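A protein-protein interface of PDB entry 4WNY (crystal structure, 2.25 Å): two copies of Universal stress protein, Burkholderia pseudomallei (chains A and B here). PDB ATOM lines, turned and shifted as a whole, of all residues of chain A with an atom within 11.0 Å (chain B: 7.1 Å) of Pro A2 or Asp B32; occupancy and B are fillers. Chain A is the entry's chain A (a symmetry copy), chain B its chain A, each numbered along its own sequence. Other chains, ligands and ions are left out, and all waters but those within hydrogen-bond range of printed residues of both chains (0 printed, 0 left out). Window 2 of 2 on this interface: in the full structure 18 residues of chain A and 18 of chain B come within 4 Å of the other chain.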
ATOM      1  N   PRO A   2     -23.921  -2.431   0.301  1.00  0.00           N
ATOM      2  CA  PRO A   2     -24.241  -2.588   1.724  1.00  0.00           C
ATOM      3  C   PRO A   2     -23.555  -3.797   2.351  1.00  0.00           C
ATOM      4  O   PRO A   2     -23.398  -4.828   1.695  1.00  0.00           O
ATOM      5  CB  PRO A   2     -25.761  -2.769   1.722  1.00  0.00           C
ATOM      6  CG  PRO A   2     -26.068  -3.330   0.383  1.00  0.00           C
ATOM      7  CD  PRO A   2     -25.087  -2.694  -0.559  1.00  0.00           C
ATOM      8  N   GLY A   3     -23.161  -3.663   3.614  1.00  0.00           N
ATOM      9  CA  GLY A   3     -22.448  -4.716   4.319  1.00  0.00           C
ATOM     10  C   GLY A   3     -23.312  -5.935   4.583  1.00  0.00           C
ATOM     11  O   GLY A   3     -24.493  -5.950   4.233  1.00  0.00           O
ATOM     12  N   SER A   4     -22.724  -6.953   5.205  1.00  0.00           N
ATOM     13  CA  SER A   4     -23.423  -8.207   5.483  1.00  0.00           C
ATOM     14  C   SER A   4     -24.014  -8.246   6.888  1.00  0.00           C
ATOM     15  O   SER A   4     -24.725  -9.189   7.243  1.00  0.00           O
ATOM     16  CB  SER A   4     -22.481  -9.400   5.302  1.00  0.00           C
ATOM     17  OG  SER A   4     -21.575  -9.519   6.389  1.00  0.00           O
ATOM     18  N   MET A   5     -23.714  -7.226   7.685  1.00  0.00           N
ATOM     19  CA  MET A   5     -24.216  -7.157   9.053  1.00  0.00           C
ATOM     20  C   MET A   5     -25.739  -7.075   9.068  1.00  0.00           C
ATOM     21  O   MET A   5     -26.388  -7.441  10.048  1.00  0.00           O
ATOM     22  CB  MET A   5     -23.614  -5.957   9.788  1.00  0.00           C
ATOM     23  CG  MET A   5     -23.977  -5.896  11.268  1.00  0.00           C
ATOM     24  SD  MET A   5     -23.253  -4.499  12.147  1.00  0.00           S
ATOM     25  CE  MET A   5     -21.502  -4.857  12.011  1.00  0.00           C
ATOM     26  N   TYR A   6     -26.303  -6.592   7.968  1.00  0.00           N
ATOM     27  CA  TYR A   6     -27.746  -6.500   7.833  1.00  0.00           C
ATOM     28  C   TYR A   6     -28.197  -7.058   6.491  1.00  0.00           C
ATOM     29  O   TYR A   6     -29.204  -6.622   5.949  1.00  0.00           O
ATOM     30  CB  TYR A   6     -28.207  -5.051   7.981  1.00  0.00           C
ATOM     31  CG  TYR A   6     -27.795  -4.408   9.285  1.00  0.00           C
ATOM     32  CD1 TYR A   6     -28.424  -4.744  10.475  1.00  0.00           C
ATOM     33  CD2 TYR A   6     -26.781  -3.460   9.323  1.00  0.00           C
ATOM     34  CE1 TYR A   6     -28.052  -4.159  11.670  1.00  0.00           C
ATOM     35  CE2 TYR A   6     -26.401  -2.868  10.514  1.00  0.00           C
ATOM     36  CZ  TYR A   6     -27.041  -3.221  11.684  1.00  0.00           C
ATOM     37  OH  TYR A   6     -26.672  -2.637  12.875  1.00  0.00           O
ATOM     38  N   SER A   7     -27.448  -8.023   5.964  1.00  0.00           N
ATOM     39  CA  SER A   7     -27.737  -8.600   4.655  1.00  0.00           C
ATOM     40  C   SER A   7     -29.046  -9.382   4.643  1.00  0.00           C
ATOM     41  O   SER A   7     -29.797  -9.335   3.669  1.00  0.00           O
ATOM     42  CB  SER A   7     -26.592  -9.509   4.210  1.00  0.00           C
ATOM     43  OG  SER A   7     -26.382 -10.549   5.150  1.00  0.00           O
ATOM     44  N   ILE A   8     -29.312 -10.105   5.728  1.00  0.00           N
ATOM     45  CA  ILE A   8     -30.523 -10.910   5.828  1.00  0.00           C
ATOM     46  C   ILE A   8     -31.312 -10.586   7.095  1.00  0.00           C
ATOM     47  O   ILE A   8     -30.836 -10.791   8.212  1.00  0.00           O
ATOM     48  CB  ILE A   8     -30.198 -12.415   5.799  1.00  0.00           C
ATOM     49  CG1 ILE A   8     -29.603 -12.802   4.443  1.00  0.00           C
ATOM     50  CG2 ILE A   8     -31.448 -13.235   6.082  1.00  0.00           C
ATOM     51  CD1 ILE A   8     -29.085 -14.226   4.383  1.00  0.00           C
ATOM     52  N   ILE A   9     -32.527 -10.080   6.908  1.00  0.00           N
ATOM     53  CA  ILE A   9     -33.366  -9.667   8.025  1.00  0.00           C
ATOM     54  C   ILE A   9     -34.542 -10.614   8.234  1.00  0.00           C
ATOM     55  O   ILE A   9     -35.240 -10.975   7.285  1.00  0.00           O
ATOM     56  CB  ILE A   9     -33.916  -8.246   7.818  1.00  0.00           C
ATOM     57  CG1 ILE A   9     -32.784  -7.280   7.454  1.00  0.00           C
ATOM     58  CG2 ILE A   9     -34.654  -7.778   9.062  1.00  0.00           C
ATOM     59  CD1 ILE A   9     -33.265  -5.885   7.110  1.00  0.00           C
ATOM     60  N   GLU A  28     -39.248  -1.629   4.955  1.00  0.00           N
ATOM     61  CA  GLU A  28     -38.651  -0.320   4.718  1.00  0.00           C
ATOM     62  C   GLU A  28     -37.152  -0.349   4.976  1.00  0.00           C
ATOM     63  O   GLU A  28     -36.374   0.270   4.251  1.00  0.00           O
ATOM     64  CB  GLU A  28     -39.313   0.741   5.601  1.00  0.00           C
ATOM     65  N   LEU A  29     -36.753  -1.075   6.014  1.00  0.00           N
ATOM     66  CA  LEU A  29     -35.343  -1.233   6.341  1.00  0.00           C
ATOM     67  C   LEU A  29     -34.640  -2.084   5.293  1.00  0.00           C
ATOM     68  O   LEU A  29     -33.522  -1.778   4.880  1.00  0.00           O
ATOM     69  CB  LEU A  29     -35.179  -1.865   7.724  1.00  0.00           C
ATOM     70  CG  LEU A  29     -33.744  -1.985   8.229  1.00  0.00           C
ATOM     71  CD1 LEU A  29     -33.202  -0.615   8.586  1.00  0.00           C
ATOM     72  CD2 LEU A  29     -33.668  -2.922   9.418  1.00  0.00           C
ATOM     73  N   ALA A  30     -35.305  -3.155   4.869  1.00  0.00           N
ATOM     74  CA  ALA A  30     -34.754  -4.059   3.867  1.00  0.00           C
ATOM     75  C   ALA A  30     -34.540  -3.349   2.534  1.00  0.00           C
ATOM     76  O   ALA A  30     -33.569  -3.618   1.827  1.00  0.00           O
ATOM     77  CB  ALA A  30     -35.666  -5.263   3.683  1.00  0.00           C
ATOM     78  N   ALA A  31     -35.451  -2.441   2.198  1.00  0.00           N
ATOM     79  CA  ALA A  31     -35.357  -1.692   0.951  1.00  0.00           C
ATOM     80  C   ALA A  31     -34.273  -0.621   1.034  1.00  0.00           C
ATOM     81  O   ALA A  31     -33.525  -0.410   0.080  1.00  0.00           O
ATOM     82  CB  ALA A  31     -36.701  -1.063   0.608  1.00  0.00           C
ATOM     83  N   ASP A  32     -34.197   0.049   2.181  1.00  0.00           N
ATOM     84  CA  ASP A  32     -33.207   1.102   2.392  1.00  0.00           C
ATOM     85  C   ASP A  32     -31.796   0.535   2.450  1.00  0.00           C
ATOM     86  O   ASP A  32     -30.862   1.107   1.891  1.00  0.00           O
ATOM     87  CB  ASP A  32     -33.506   1.877   3.679  1.00  0.00           C
ATOM     88  CG  ASP A  32     -34.693   2.809   3.538  1.00  0.00           C
ATOM     89  OD1 ASP A  32     -35.134   3.033   2.391  1.00  0.00           O
ATOM     90  OD2 ASP A  32     -35.177   3.327   4.566  1.00  0.00           O
ATOM     91  N   ALA A  33     -31.647  -0.596   3.131  1.00  0.00           N
ATOM     92  CA  ALA A  33     -30.340  -1.217   3.290  1.00  0.00           C
ATOM     93  C   ALA A  33     -30.049  -2.209   2.173  1.00  0.00           C
ATOM     94  O   ALA A  33     -29.006  -2.865   2.179  1.00  0.00           O
ATOM     95  CB  ALA A  33     -30.244  -1.904   4.641  1.00  0.00           C
ATOM     96  N   HIS A  34     -30.976  -2.308   1.220  1.00  0.00           N
ATOM     97  CA  HIS A  34     -30.853  -3.229   0.093  1.00  0.00           C
ATOM     98  C   HIS A  34     -30.628  -4.648   0.592  1.00  0.00           C
ATOM     99  O   HIS A  34     -29.755  -5.365   0.100  1.00  0.00           O
ATOM    100  CB  HIS A  34     -29.715  -2.807  -0.838  1.00  0.00           C
ATOM    101  CG  HIS A  34     -29.959  -1.508  -1.537  1.00  0.00           C
ATOM    102  ND1 HIS A  34     -30.414  -0.382  -0.884  1.00  0.00           N
ATOM    103  CD2 HIS A  34     -29.807  -1.153  -2.835  1.00  0.00           C
ATOM    104  CE1 HIS A  34     -30.535   0.609  -1.750  1.00  0.00           C
ATOM    105  NE2 HIS A  34     -30.171   0.167  -2.940  1.00  0.00           N
ATOM    106  N   ALA A  35     -31.428  -5.041   1.575  1.00  0.00           N
ATOM    107  CA  ALA A  35     -31.235  -6.307   2.262  1.00  0.00           C
ATOM    108  C   ALA A  35     -32.281  -7.342   1.876  1.00  0.00           C
ATOM    109  O   ALA A  35     -33.342  -7.007   1.349  1.00  0.00           O
ATOM    110  CB  ALA A  35     -31.254  -6.084   3.759  1.00  0.00           C
ATOM    111  N   ARG A  36     -31.970  -8.606   2.140  1.00  0.00           N
ATOM    112  CA  ARG A  36     -32.932  -9.681   1.952  1.00  0.00           C
ATOM    113  C   ARG A  36     -33.831  -9.789   3.176  1.00  0.00           C
ATOM    114  O   ARG A  36     -33.359  -9.728   4.310  1.00  0.00           O
ATOM    115  CB  ARG A  36     -32.218 -11.010   1.703  1.00  0.00           C
ATOM    116  CG  ARG A  36     -31.404 -11.050   0.423  1.00  0.00           C
ATOM    117  CD  ARG A  36     -30.706 -12.390   0.267  1.00  0.00           C
ATOM    118  NE  ARG A  36     -31.658 -13.493   0.179  1.00  0.00           N
ATOM    119  CZ  ARG A  36     -32.158 -13.957  -0.961  1.00  0.00           C
ATOM    120  NH1 ARG A  36     -31.796 -13.414  -2.115  1.00  0.00           N
ATOM    121  NH2 ARG A  36     -33.019 -14.965  -0.948  1.00  0.00           N
ATOM    122  N   SER A 114     -29.003 -12.010  10.425  1.00  0.00           N
ATOM    123  CA  SER A 114     -28.141 -11.224  11.294  1.00  0.00           C
ATOM    124  C   SER A 114     -28.966 -10.218  12.087  1.00  0.00           C
ATOM    125  O   SER A 114     -28.426  -9.410  12.844  1.00  0.00           O
ATOM    126  CB  SER A 114     -27.065 -10.512  10.474  1.00  0.00           C
ATOM    127  OG  SER A 114     -27.642  -9.801   9.393  1.00  0.00           O
ATOM    128  N   LEU A 115     -30.282 -10.278  11.911  1.00  0.00           N
ATOM    129  CA  LEU A 115     -31.200  -9.379  12.600  1.00  0.00           C
ATOM    130  C   LEU A 115     -32.597  -9.980  12.705  1.00  0.00           C
ATOM    131  O   LEU A 115     -33.103 -10.563  11.746  1.00  0.00           O
ATOM    132  CB  LEU A 115     -31.271  -8.030  11.882  1.00  0.00           C
ATOM    133  CG  LEU A 115     -32.281  -7.023  12.441  1.00  0.00           C
ATOM    134  CD1 LEU A 115     -31.907  -6.617  13.861  1.00  0.00           C
ATOM    135  CD2 LEU A 115     -32.388  -5.806  11.533  1.00  0.00           C
ATOM    136  N   PRO B   2     -33.533   6.776   0.392  1.00  0.00           N
ATOM    137  CA  PRO B   2     -34.002   6.083   1.597  1.00  0.00           C
ATOM    138  C   PRO B   2     -35.097   6.852   2.329  1.00  0.00           C
ATOM    139  O   PRO B   2     -35.068   8.083   2.367  1.00  0.00           O
ATOM    140  CB  PRO B   2     -32.741   5.985   2.458  1.00  0.00           C
ATOM    141  CG  PRO B   2     -31.898   7.123   2.014  1.00  0.00           C
ATOM    142  CD  PRO B   2     -32.154   7.269   0.542  1.00  0.00           C
ATOM    143  N   ALA B  26     -24.530   0.561  14.694  1.00  0.00           N
ATOM    144  CA  ALA B  26     -25.345   1.716  14.335  1.00  0.00           C
ATOM    145  C   ALA B  26     -24.725   2.469  13.163  1.00  0.00           C
ATOM    146  O   ALA B  26     -25.435   2.971  12.293  1.00  0.00           O
ATOM    147  CB  ALA B  26     -25.516   2.640  15.532  1.00  0.00           C
ATOM    148  N   LEU B  27     -23.397   2.541  13.147  1.00  0.00           N
ATOM    149  CA  LEU B  27     -22.677   3.171  12.046  1.00  0.00           C
ATOM    150  C   LEU B  27     -22.897   2.417  10.745  1.00  0.00           C
ATOM    151  O   LEU B  27     -23.200   3.017   9.714  1.00  0.00           O
ATOM    152  CB  LEU B  27     -21.180   3.248  12.349  1.00  0.00           C
ATOM    153  CG  LEU B  27     -20.633   4.602  12.792  1.00  0.00           C
ATOM    154  CD1 LEU B  27     -19.130   4.523  12.945  1.00  0.00           C
ATOM    155  CD2 LEU B  27     -21.008   5.681  11.794  1.00  0.00           C
ATOM    156  N   GLU B  28     -22.733   1.098  10.801  1.00  0.00           N
ATOM    157  CA  GLU B  28     -22.908   0.244   9.632  1.00  0.00           C
ATOM    158  C   GLU B  28     -24.314   0.373   9.068  1.00  0.00           C
ATOM    159  O   GLU B  28     -24.509   0.382   7.853  1.00  0.00           O
ATOM    160  CB  GLU B  28     -22.616  -1.217   9.985  1.00  0.00           C
ATOM    161  N   LEU B  29     -25.293   0.474   9.960  1.00  0.00           N
ATOM    162  CA  LEU B  29     -26.680   0.657   9.557  1.00  0.00           C
ATOM    163  C   LEU B  29     -26.888   2.041   8.958  1.00  0.00           C
ATOM    164  O   LEU B  29     -27.579   2.194   7.951  1.00  0.00           O
ATOM    165  CB  LEU B  29     -27.618   0.455  10.747  1.00  0.00           C
ATOM    166  CG  LEU B  29     -29.110   0.514  10.430  1.00  0.00           C
ATOM    167  CD1 LEU B  29     -29.526  -0.720   9.657  1.00  0.00           C
ATOM    168  CD2 LEU B  29     -29.925   0.656  11.702  1.00  0.00           C
ATOM    169  N   ALA B  30     -26.285   3.045   9.586  1.00  0.00           N
ATOM    170  CA  ALA B  30     -26.396   4.423   9.125  1.00  0.00           C
ATOM    171  C   ALA B  30     -25.792   4.595   7.735  1.00  0.00           C
ATOM    172  O   ALA B  30     -26.304   5.358   6.916  1.00  0.00           O
ATOM    173  CB  ALA B  30     -25.725   5.367  10.111  1.00  0.00           C
ATOM    174  N   ALA B  31     -24.702   3.880   7.475  1.00  0.00           N
ATOM    175  CA  ALA B  31     -24.032   3.953   6.182  1.00  0.00           C
ATOM    176  C   ALA B  31     -24.819   3.201   5.113  1.00  0.00           C
ATOM    177  O   ALA B  31     -24.941   3.665   3.979  1.00  0.00           O
ATOM    178  CB  ALA B  31     -22.616   3.401   6.286  1.00  0.00           C
ATOM    179  N   ASP B  32     -25.352   2.039   5.483  1.00  0.00           N
ATOM    180  CA  ASP B  32     -26.127   1.218   4.558  1.00  0.00           C
ATOM    181  C   ASP B  32     -27.446   1.884   4.194  1.00  0.00           C
ATOM    182  O   ASP B  32     -27.864   1.867   3.037  1.00  0.00           O
ATOM    183  CB  ASP B  32     -26.394  -0.167   5.154  1.00  0.00           C
ATOM    184  CG  ASP B  32     -25.164  -1.052   5.151  1.00  0.00           C
ATOM    185  OD1 ASP B  32     -24.176  -0.688   4.480  1.00  0.00           O
ATOM    186  OD2 ASP B  32     -25.186  -2.116   5.807  1.00  0.00           O
ATOM    187  N   ALA B  33     -28.099   2.472   5.190  1.00  0.00           N
ATOM    188  CA  ALA B  33     -29.390   3.110   4.977  1.00  0.00           C
ATOM    189  C   ALA B  33     -29.236   4.581   4.615  1.00  0.00           C
ATOM    190  O   ALA B  33     -30.232   5.288   4.450  1.00  0.00           O
ATOM    191  CB  ALA B  33     -30.262   2.961   6.210  1.00  0.00           C
ATOM    192  N   HIS B  34     -27.987   5.028   4.493  1.00  0.00           N
ATOM    193  CA  HIS B  34     -27.674   6.419   4.171  1.00  0.00           C
ATOM    194  C   HIS B  34     -28.347   7.355   5.162  1.00  0.00           C
ATOM    195  O   HIS B  34     -28.957   8.354   4.780  1.00  0.00           O
ATOM    196  CB  HIS B  34     -28.103   6.759   2.744  1.00  0.00           C
ATOM    197  CG  HIS B  34     -27.333   6.027   1.691  1.00  0.00           C
ATOM    198  ND1 HIS B  34     -27.092   4.671   1.751  1.00  0.00           N
ATOM    199  CD2 HIS B  34     -26.751   6.462   0.548  1.00  0.00           C
ATOM    200  CE1 HIS B  34     -26.393   4.303   0.691  1.00  0.00           C
ATOM    201  NE2 HIS B  34     -26.174   5.371  -0.054  1.00  0.00           N
ATOM    202  N   ALA B  35     -28.226   7.017   6.440  1.00  0.00           N
ATOM    203  CA  ALA B  35     -28.942   7.719   7.491  1.00  0.00           C
ATOM    204  C   ALA B  35     -28.028   8.612   8.318  1.00  0.00           C
ATOM    205  O   ALA B  35     -26.808   8.449   8.315  1.00  0.00           O
ATOM    206  CB  ALA B  35     -29.642   6.722   8.388  1.00  0.00           C
ATOM    207  N   VAL B  84     -20.465   9.141   7.485  1.00  0.00           N
ATOM    208  CA  VAL B  84     -21.819   9.184   8.025  1.00  0.00           C
ATOM    209  C   VAL B  84     -22.118  10.542   8.650  1.00  0.00           C
ATOM    210  O   VAL B  84     -21.375  11.017   9.508  1.00  0.00           O
ATOM    211  CB  VAL B  84     -22.040   8.086   9.080  1.00  0.00           C
ATOM    212  CG1 VAL B  84     -23.358   8.302   9.812  1.00  0.00           C
ATOM    213  CG2 VAL B  84     -21.992   6.710   8.432  1.00  0.00           C
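OD1 of Asp B32 is in hydrogen-bond range of N of Gly A3 (3.3 Å).
The backbone carbonyl oxygen of Asp B32 sits close to the backbone carbonyl oxygen of Asp A32, at 3.3 Å.
The backbone carbonyl oxygen (O) of Met A5 is in hydrogen-bond range of the side-chain hydroxyl (OG) of Ser A114, at 2.8 Å.
O of Asp A32 sits at hydrogen-bond distance from ND1 of His A34 (3.2 Å).
O of Asp B32 sits at hydrogen-bond distance from ND1 of His B34 (3.2 Å).
CA of Pro A2 touches OD1 of Asp B32, 3.3 Å away.
CB of Glu B28 touches SD of Met A5 (3.98 Å).
Tyr A6 touches Leu B29.
Leu B29 touches Leu A29.
CA of Pro B2 touches OD1 of Asp A32, at 3.3 Å.
Asp A32 touches Ala B33.
Ala A33 touches Asp B32 (CA to O, 3.96 Å).
Pro A2 touches just one residue of chain B: Asp B32.
Printed residues of chain B within 4 Å of Met A5: Glu B28.
Of the printed residues of chain B, Tyr A6 touches Leu B29.
Ile A9 touches none of the printed residues of chain B.
Printed residues of chain B within 4 Å of Asp A32: Pro B2, Asp B32 and Ala B33.
Of the printed residues of chain A, Pro B2 touches Asp A32 (3.3 Å).
Of the printed residues of chain A, Leu B29 touches Tyr A6 (3.5 Å) and Leu A29 (3.8 Å).
Ala B30 touches none of the printed residues of chain A.
No residue of chain A comes within 4 Å of Ala B31.
Of the printed residues of chain A, Ala B33 touches Asp A32.
His B34 touches none of the printed residues of chain A.
Ala B35 touches none of the printed residues of chain A.
The nearest residue of chain A that does not touch Asp B32 is Tyr A6 (4.1 Å).
Hydrophobic or aromatic side chains of chain A that line the printed part of chain B: Pro A2, Met A5, Tyr A6 and Leu A29.
Of the 12 printed residues of chain B, 5 touch a printed residue of chain A.
Printed residues of chain B that touch a printed residue of chain A: Pro B2, Glu B28, Leu B29, Asp B32 and Ala B33.
Hydrophobic or aromatic side chains of chain B within 4 Å of the printed part of chain A: Pro B2 and Leu B29.
Pro A2 touches Asp B32, and with the chains exchanged Asp A32 touches Pro B2.
Leu B29 touches its own counterpart, Leu A29.
Asp B32 touches its own counterpart, Asp A32.
Asp A32 touches Ala B33, and with the chains exchanged Ala A33 touches Asp B32.
Positions printed for both chains: 2, 28, 29, 30, 31, 32, 33, 34 and 35.
Of the 9 pairs that touch across the chains among the printed residues, 6 have their exchanged pair printed and touching as well.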
